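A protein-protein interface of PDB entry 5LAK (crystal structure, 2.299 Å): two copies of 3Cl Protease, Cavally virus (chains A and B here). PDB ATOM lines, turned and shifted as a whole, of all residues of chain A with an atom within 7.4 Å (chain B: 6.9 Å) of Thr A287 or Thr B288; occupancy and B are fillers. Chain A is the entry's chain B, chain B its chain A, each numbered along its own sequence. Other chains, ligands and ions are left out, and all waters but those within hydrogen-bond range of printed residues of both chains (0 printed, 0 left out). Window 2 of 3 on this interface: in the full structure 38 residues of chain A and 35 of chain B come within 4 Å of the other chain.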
ATOM      1  N   ASN A 281      -3.370   0.122  11.868  1.00  0.00           N
ATOM      2  CA  ASN A 281      -1.944   0.424  11.891  1.00  0.00           C
ATOM      3  C   ASN A 281      -1.126  -0.824  12.205  1.00  0.00           C
ATOM      4  O   ASN A 281      -0.025  -0.734  12.746  1.00  0.00           O
ATOM      5  CB  ASN A 281      -1.649   1.520  12.915  1.00  0.00           C
ATOM      6  CG  ASN A 281      -2.283   2.847  12.548  1.00  0.00           C
ATOM      7  OD1 ASN A 281      -1.783   3.568  11.684  1.00  0.00           O
ATOM      8  ND2 ASN A 281      -3.391   3.175  13.204  1.00  0.00           N
ATOM      9  N   PHE A 282      -1.678  -1.985  11.857  1.00  0.00           N
ATOM     10  CA  PHE A 282      -1.087  -3.273  12.216  1.00  0.00           C
ATOM     11  C   PHE A 282       0.379  -3.381  11.809  1.00  0.00           C
ATOM     12  O   PHE A 282       1.233  -3.736  12.621  1.00  0.00           O
ATOM     13  CB  PHE A 282      -1.878  -4.411  11.569  1.00  0.00           C
ATOM     14  CG  PHE A 282      -1.309  -5.771  11.842  1.00  0.00           C
ATOM     15  CD1 PHE A 282      -1.418  -6.346  13.097  1.00  0.00           C
ATOM     16  CD2 PHE A 282      -0.652  -6.472  10.842  1.00  0.00           C
ATOM     17  CE1 PHE A 282      -0.891  -7.599  13.349  1.00  0.00           C
ATOM     18  CE2 PHE A 282      -0.124  -7.723  11.084  1.00  0.00           C
ATOM     19  CZ  PHE A 282      -0.241  -8.289  12.342  1.00  0.00           C
ATOM     20  N   ASN A 283       0.658  -3.067  10.549  1.00  0.00           N
ATOM     21  CA  ASN A 283       1.997  -3.209  10.000  1.00  0.00           C
ATOM     22  C   ASN A 283       3.015  -2.324  10.711  1.00  0.00           C
ATOM     23  O   ASN A 283       4.118  -2.768  11.034  1.00  0.00           O
ATOM     24  CB  ASN A 283       1.981  -2.891   8.507  1.00  0.00           C
ATOM     25  CG  ASN A 283       3.352  -2.987   7.879  1.00  0.00           C
ATOM     26  OD1 ASN A 283       3.986  -4.044   7.889  1.00  0.00           O
ATOM     27  ND2 ASN A 283       3.821  -1.876   7.318  1.00  0.00           N
ATOM     28  N   ARG A 284       2.639  -1.073  10.952  1.00  0.00           N
ATOM     29  CA  ARG A 284       3.507  -0.126  11.639  1.00  0.00           C
ATOM     30  C   ARG A 284       3.773  -0.569  13.073  1.00  0.00           C
ATOM     31  O   ARG A 284       4.919  -0.586  13.527  1.00  0.00           O
ATOM     32  CB  ARG A 284       2.884   1.275  11.633  1.00  0.00           C
ATOM     33  CG  ARG A 284       3.736   2.353  12.300  1.00  0.00           C
ATOM     34  CD  ARG A 284       3.294   3.744  11.875  1.00  0.00           C
ATOM     35  NE  ARG A 284       1.933   4.055  12.312  1.00  0.00           N
ATOM     36  CZ  ARG A 284       1.613   4.522  13.515  1.00  0.00           C
ATOM     37  NH1 ARG A 284       2.555   4.759  14.420  1.00  0.00           N
ATOM     38  NH2 ARG A 284       0.342   4.769  13.813  1.00  0.00           N
ATOM     39  N   TYR A 285       2.708  -0.934  13.776  1.00  0.00           N
ATOM     40  CA  TYR A 285       2.807  -1.286  15.186  1.00  0.00           C
ATOM     41  C   TYR A 285       3.603  -2.568  15.433  1.00  0.00           C
ATOM     42  O   TYR A 285       4.233  -2.708  16.476  1.00  0.00           O
ATOM     43  CB  TYR A 285       1.404  -1.423  15.795  1.00  0.00           C
ATOM     44  CG  TYR A 285       0.659  -0.112  16.007  1.00  0.00           C
ATOM     45  CD1 TYR A 285       1.333   1.104  16.065  1.00  0.00           C
ATOM     46  CD2 TYR A 285      -0.722  -0.097  16.171  1.00  0.00           C
ATOM     47  CE1 TYR A 285       0.654   2.293  16.263  1.00  0.00           C
ATOM     48  CE2 TYR A 285      -1.407   1.086  16.373  1.00  0.00           C
ATOM     49  CZ  TYR A 285      -0.716   2.278  16.418  1.00  0.00           C
ATOM     50  OH  TYR A 285      -1.398   3.458  16.617  1.00  0.00           O
ATOM     51  N   THR A 286       3.580  -3.502  14.487  1.00  0.00           N
ATOM     52  CA  THR A 286       4.270  -4.779  14.677  1.00  0.00           C
ATOM     53  C   THR A 286       5.692  -4.784  14.117  1.00  0.00           C
ATOM     54  O   THR A 286       6.428  -5.743  14.322  1.00  0.00           O
ATOM     55  CB  THR A 286       3.494  -5.940  14.030  1.00  0.00           C
ATOM     56  OG1 THR A 286       3.292  -5.679  12.637  1.00  0.00           O
ATOM     57  CG2 THR A 286       2.153  -6.129  14.718  1.00  0.00           C
ATOM     58  N   THR A 287       6.076  -3.711  13.428  1.00  0.00           N
ATOM     59  CA  THR A 287       7.410  -3.603  12.833  1.00  0.00           C
ATOM     60  C   THR A 287       8.214  -2.438  13.413  1.00  0.00           C
ATOM     61  O   THR A 287       9.375  -2.243  13.061  1.00  0.00           O
ATOM     62  CB  THR A 287       7.321  -3.420  11.309  1.00  0.00           C
ATOM     63  OG1 THR A 287       6.581  -2.229  11.015  1.00  0.00           O
ATOM     64  CG2 THR A 287       6.628  -4.613  10.661  1.00  0.00           C
ATOM     65  N   THR A 288       7.590  -1.678  14.305  1.00  0.00           N
ATOM     66  CA  THR A 288       8.228  -0.536  14.947  1.00  0.00           C
ATOM     67  C   THR A 288       8.440  -0.858  16.416  1.00  0.00           C
ATOM     68  O   THR A 288       7.639  -1.571  17.019  1.00  0.00           O
ATOM     69  CB  THR A 288       7.365   0.743  14.791  1.00  0.00           C
ATOM     70  OG1 THR A 288       7.204   1.040  13.401  1.00  0.00           O
ATOM     71  CG2 THR A 288       8.000   1.944  15.483  1.00  0.00           C
ATOM     72  N   THR A 289       9.512  -0.330  16.997  1.00  0.00           N
ATOM     73  CA  THR A 289       9.851  -0.647  18.379  1.00  0.00           C
ATOM     74  C   THR A 289       9.085   0.264  19.330  1.00  0.00           C
ATOM     75  O   THR A 289       8.687   1.366  18.953  1.00  0.00           O
ATOM     76  CB  THR A 289      11.360  -0.496  18.650  1.00  0.00           C
ATOM     77  OG1 THR A 289      11.805   0.789  18.199  1.00  0.00           O
ATOM     78  CG2 THR A 289      12.151  -1.585  17.941  1.00  0.00           C
ATOM     79  N   SER A 294      11.040  -4.601  20.754  1.00  0.00           N
ATOM     80  CA  SER A 294      10.219  -5.112  19.667  1.00  0.00           C
ATOM     81  C   SER A 294       8.817  -5.428  20.166  1.00  0.00           C
ATOM     82  O   SER A 294       8.610  -5.650  21.358  1.00  0.00           O
ATOM     83  CB  SER A 294      10.849  -6.366  19.068  1.00  0.00           C
ATOM     84  OG  SER A 294      10.703  -7.466  19.953  1.00  0.00           O
ATOM     85  N   PHE A 295       7.862  -5.462  19.247  1.00  0.00           N
ATOM     86  CA  PHE A 295       6.485  -5.794  19.588  1.00  0.00           C
ATOM     87  C   PHE A 295       6.417  -7.186  20.208  1.00  0.00           C
ATOM     88  O   PHE A 295       5.744  -7.385  21.216  1.00  0.00           O
ATOM     89  CB  PHE A 295       5.592  -5.707  18.346  1.00  0.00           C
ATOM     90  CG  PHE A 295       4.151  -6.056  18.599  1.00  0.00           C
ATOM     91  CD1 PHE A 295       3.276  -5.111  19.108  1.00  0.00           C
ATOM     92  CD2 PHE A 295       3.667  -7.322  18.313  1.00  0.00           C
ATOM     93  CE1 PHE A 295       1.943  -5.424  19.333  1.00  0.00           C
ATOM     94  CE2 PHE A 295       2.341  -7.641  18.537  1.00  0.00           C
ATOM     95  CZ  PHE A 295       1.477  -6.690  19.046  1.00  0.00           C
ATOM     96  N   LEU B 241      21.665  -4.337   6.372  1.00  0.00           N
ATOM     97  CA  LEU B 241      20.742  -3.238   6.101  1.00  0.00           C
ATOM     98  C   LEU B 241      21.101  -2.461   4.842  1.00  0.00           C
ATOM     99  O   LEU B 241      20.214  -1.997   4.131  1.00  0.00           O
ATOM    100  CB  LEU B 241      20.691  -2.262   7.280  1.00  0.00           C
ATOM    101  CG  LEU B 241      20.010  -2.757   8.553  1.00  0.00           C
ATOM    102  CD1 LEU B 241      20.281  -1.797   9.708  1.00  0.00           C
ATOM    103  CD2 LEU B 241      18.516  -2.920   8.322  1.00  0.00           C
ATOM    104  N   ASN B 283      16.885   6.913  11.015  1.00  0.00           N
ATOM    105  CA  ASN B 283      15.710   6.816  11.866  1.00  0.00           C
ATOM    106  C   ASN B 283      14.912   5.542  11.624  1.00  0.00           C
ATOM    107  O   ASN B 283      14.502   4.869  12.573  1.00  0.00           O
ATOM    108  CB  ASN B 283      14.805   8.023  11.656  1.00  0.00           C
ATOM    109  CG  ASN B 283      13.563   7.959  12.511  1.00  0.00           C
ATOM    110  OD1 ASN B 283      13.643   7.937  13.738  1.00  0.00           O
ATOM    111  ND2 ASN B 283      12.402   7.908  11.869  1.00  0.00           N
ATOM    112  N   ARG B 284      14.693   5.211  10.356  1.00  0.00           N
ATOM    113  CA  ARG B 284      13.947   4.007  10.012  1.00  0.00           C
ATOM    114  C   ARG B 284      14.691   2.759  10.485  1.00  0.00           C
ATOM    115  O   ARG B 284      14.095   1.859  11.075  1.00  0.00           O
ATOM    116  CB  ARG B 284      13.696   3.921   8.508  1.00  0.00           C
ATOM    117  CG  ARG B 284      12.879   2.702   8.128  1.00  0.00           C
ATOM    118  CD  ARG B 284      12.267   2.828   6.754  1.00  0.00           C
ATOM    119  NE  ARG B 284      13.280   2.894   5.704  1.00  0.00           N
ATOM    120  CZ  ARG B 284      13.886   1.831   5.179  1.00  0.00           C
ATOM    121  NH1 ARG B 284      13.600   0.609   5.612  1.00  0.00           N
ATOM    122  NH2 ARG B 284      14.791   1.994   4.225  1.00  0.00           N
ATOM    123  N   TYR B 285      15.995   2.711  10.225  1.00  0.00           N
ATOM    124  CA  TYR B 285      16.794   1.539  10.564  1.00  0.00           C
ATOM    125  C   TYR B 285      16.891   1.306  12.072  1.00  0.00           C
ATOM    126  O   TYR B 285      16.999   0.161  12.515  1.00  0.00           O
ATOM    127  CB  TYR B 285      18.205   1.668   9.968  1.00  0.00           C
ATOM    128  CG  TYR B 285      18.301   1.429   8.468  1.00  0.00           C
ATOM    129  CD1 TYR B 285      17.332   0.701   7.789  1.00  0.00           C
ATOM    130  CD2 TYR B 285      19.376   1.921   7.733  1.00  0.00           C
ATOM    131  CE1 TYR B 285      17.423   0.476   6.431  1.00  0.00           C
ATOM    132  CE2 TYR B 285      19.474   1.701   6.368  1.00  0.00           C
ATOM    133  CZ  TYR B 285      18.492   0.976   5.724  1.00  0.00           C
ATOM    134  OH  TYR B 285      18.570   0.745   4.369  1.00  0.00           O
ATOM    135  N   THR B 286      16.849   2.376  12.857  1.00  0.00           N
ATOM    136  CA  THR B 286      16.982   2.258  14.308  1.00  0.00           C
ATOM    137  C   THR B 286      15.646   2.168  15.057  1.00  0.00           C
ATOM    138  O   THR B 286      15.644   1.985  16.280  1.00  0.00           O
ATOM    139  CB  THR B 286      17.791   3.431  14.894  1.00  0.00           C
ATOM    140  OG1 THR B 286      17.186   4.676  14.527  1.00  0.00           O
ATOM    141  CG2 THR B 286      19.225   3.385  14.388  1.00  0.00           C
ATOM    142  N   THR B 287      14.526   2.318  14.349  1.00  0.00           N
ATOM    143  CA  THR B 287      13.211   2.220  14.989  1.00  0.00           C
ATOM    144  C   THR B 287      12.343   1.094  14.430  1.00  0.00           C
ATOM    145  O   THR B 287      11.261   0.830  14.953  1.00  0.00           O
ATOM    146  CB  THR B 287      12.419   3.530  14.839  1.00  0.00           C
ATOM    147  OG1 THR B 287      12.218   3.804  13.447  1.00  0.00           O
ATOM    148  CG2 THR B 287      13.157   4.690  15.486  1.00  0.00           C
ATOM    149  N   THR B 288      12.808   0.441  13.369  1.00  0.00           N
ATOM    150  CA  THR B 288      12.079  -0.678  12.776  1.00  0.00           C
ATOM    151  C   THR B 288      12.905  -1.948  12.958  1.00  0.00           C
ATOM    152  O   THR B 288      14.136  -1.896  12.997  1.00  0.00           O
ATOM    153  CB  THR B 288      11.750  -0.441  11.290  1.00  0.00           C
ATOM    154  OG1 THR B 288      12.955  -0.399  10.522  1.00  0.00           O
ATOM    155  CG2 THR B 288      10.985   0.865  11.120  1.00  0.00           C
ATOM    156  N   THR B 289      12.234  -3.087  13.070  1.00  0.00           N
ATOM    157  CA  THR B 289      12.921  -4.334  13.384  1.00  0.00           C
ATOM    158  C   THR B 289      13.517  -5.025  12.163  1.00  0.00           C
ATOM    159  O   THR B 289      13.082  -4.817  11.030  1.00  0.00           O
ATOM    160  CB  THR B 289      11.975  -5.339  14.086  1.00  0.00           C
ATOM    161  OG1 THR B 289      10.766  -5.481  13.334  1.00  0.00           O
ATOM    162  CG2 THR B 289      11.642  -4.866  15.499  1.00  0.00           C
ATOM    163  N   ILE B 290      14.530  -5.843  12.429  1.00  0.00           N
ATOM    164  CA  ILE B 290      15.108  -6.744  11.444  1.00  0.00           C
ATOM    165  C   ILE B 290      14.574  -8.109  11.816  1.00  0.00           C
ATOM    166  O   ILE B 290      14.947  -8.673  12.841  1.00  0.00           O
ATOM    167  CB  ILE B 290      16.649  -6.734  11.470  1.00  0.00           C
ATOM    168  CG1 ILE B 290      17.178  -5.330  11.178  1.00  0.00           C
ATOM    169  CG2 ILE B 290      17.211  -7.725  10.456  1.00  0.00           C
ATOM    170  CD1 ILE B 290      18.662  -5.161  11.458  1.00  0.00           C
ATOM    171  N   GLY B 291      13.682  -8.635  10.987  1.00  0.00           N
ATOM    172  CA  GLY B 291      12.851  -9.742  11.416  1.00  0.00           C
ATOM    173  C   GLY B 291      11.942  -9.197  12.503  1.00  0.00           C
ATOM    174  O   GLY B 291      11.137  -8.296  12.251  1.00  0.00           O
ATOM    175  N   LYS B 293      13.664  -8.605  15.500  1.00  0.00           N
ATOM    176  CA  LYS B 293      14.736  -8.121  16.364  1.00  0.00           C
ATOM    177  C   LYS B 293      14.873  -6.602  16.291  1.00  0.00           C
ATOM    178  O   LYS B 293      14.819  -6.022  15.206  1.00  0.00           O
ATOM    179  CB  LYS B 293      16.069  -8.765  15.976  1.00  0.00           C
ATOM    180  CG  LYS B 293      16.047 -10.283  15.897  1.00  0.00           C
ATOM    181  CD  LYS B 293      17.324 -10.822  15.255  1.00  0.00           C
ATOM    182  CE  LYS B 293      17.350 -10.595  13.748  1.00  0.00           C
ATOM    183  NZ  LYS B 293      16.344 -11.432  13.042  1.00  0.00           N
ATOM    184  N   SER B 294      15.055  -5.966  17.445  1.00  0.00           N
ATOM    185  CA  SER B 294      15.362  -4.541  17.494  1.00  0.00           C
ATOM    186  C   SER B 294      16.782  -4.295  17.005  1.00  0.00           C
ATOM    187  O   SER B 294      17.620  -5.195  17.032  1.00  0.00           O
ATOM    188  CB  SER B 294      15.215  -3.999  18.915  1.00  0.00           C
ATOM    189  OG  SER B 294      16.290  -4.435  19.730  1.00  0.00           O
ATOM    190  N   PHE B 295      17.050  -3.070  16.568  1.00  0.00           N
ATOM    191  CA  PHE B 295      18.389  -2.696  16.132  1.00  0.00           C
ATOM    192  C   PHE B 295      19.391  -2.871  17.277  1.00  0.00           C
ATOM    193  O   PHE B 295      20.500  -3.375  17.077  1.00  0.00           O
ATOM    194  CB  PHE B 295      18.402  -1.256  15.610  1.00  0.00           C
ATOM    195  CG  PHE B 295      19.758  -0.780  15.169  1.00  0.00           C
ATOM    196  CD1 PHE B 295      20.240  -1.097  13.908  1.00  0.00           C
ATOM    197  CD2 PHE B 295      20.546  -0.009  16.009  1.00  0.00           C
ATOM    198  CE1 PHE B 295      21.485  -0.657  13.496  1.00  0.00           C
ATOM    199  CE2 PHE B 295      21.793   0.432  15.603  1.00  0.00           C
ATOM    200  CZ  PHE B 295      22.262   0.109  14.346  1.00  0.00           C
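Phe A282 touches none of the printed residues of chain B.
Tyr A285 touches none of the printed residues of chain B.
Thr A287 touches just these residues of chain B: Thr B288 (3.1 Å) and Thr B289 (3.0 Å).
Printed residues of chain B within 4 Å of Thr A288: Thr B287.
Of the printed residues of chain B, Thr A289 touches Thr B287 (2.9 Å).
Of chain A, only Thr A287 (3.1 Å) comes within 4 Å of Thr B288.
Of the printed residues of chain A, Thr B289 touches Thr A287 (3.0 Å) and Ser A294 (3.95 Å).
The nearest residue of chain B that does not touch Thr A287 is Thr B287 (4.1 Å).
The nearest residue of chain A that does not touch Thr B288 is Thr A288 (4.4 Å).
The nearest printed residue of chain A that does not touch Thr B289 is Thr A289 (4.1 Å).
Of the 11 printed residues of chain A, 4 touch a printed residue of chain B.
Printed residues of chain A that touch a printed residue of chain B: Thr A287, Thr A288, Thr A289 and Ser A294.
Along chain A the printed residues that touch a printed residue of chain B span positions 287 to 294.
Among the printed residues, 5 pairs touch across the chains.
Thr A287 touches Thr B288, and with the chains exchanged Thr A288 touches Thr B287.
Thr A287 touches Thr B289, and with the chains exchanged Thr A289 touches Thr B287.
Ser A294 touches Thr B289, but with the chains exchanged Thr A289 does not touch Ser B294 (4.02 Å).
9 positions are printed for both chains.
Thr A287 touches Thr B288 (O to CA, 3.1 Å).
Thr A288 touches Thr B287.
Ser A294 touches Thr B289 (CB to CG2, 3.95 Å).
The backbone carbonyl oxygen of Arg A284 sits at hydrogen-bond distance from the side-chain hydroxyl of Thr A288 (2.8 Å).
O of Arg A284 sits at hydrogen-bond distance from OG1 of Thr A287.
The backbone carbonyl oxygen (O) of Gly B291 lies within hydrogen-bond range of the side-chain hydroxyl (OG1) of Thr B289 (3.0 Å).
The backbone carbonyl oxygen (O) of Asn B283 lies within hydrogen-bond range of the side-chain hydroxyl (OG1) of Thr B287, at 2.7 Å.
O of Asn A283 sits at hydrogen-bond distance from OG1 of Thr A287 (2.5 Å).
O of Arg B284 sits at hydrogen-bond distance from OG1 of Thr B288.
The backbone NH of Thr A289 is in hydrogen-bond range of the backbone carbonyl oxygen of Thr B287 (2.9 Å).
The backbone NH (N) of Thr B289 lies within hydrogen-bond range of the backbone carbonyl oxygen (O) of Thr A287 (3.0 Å).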
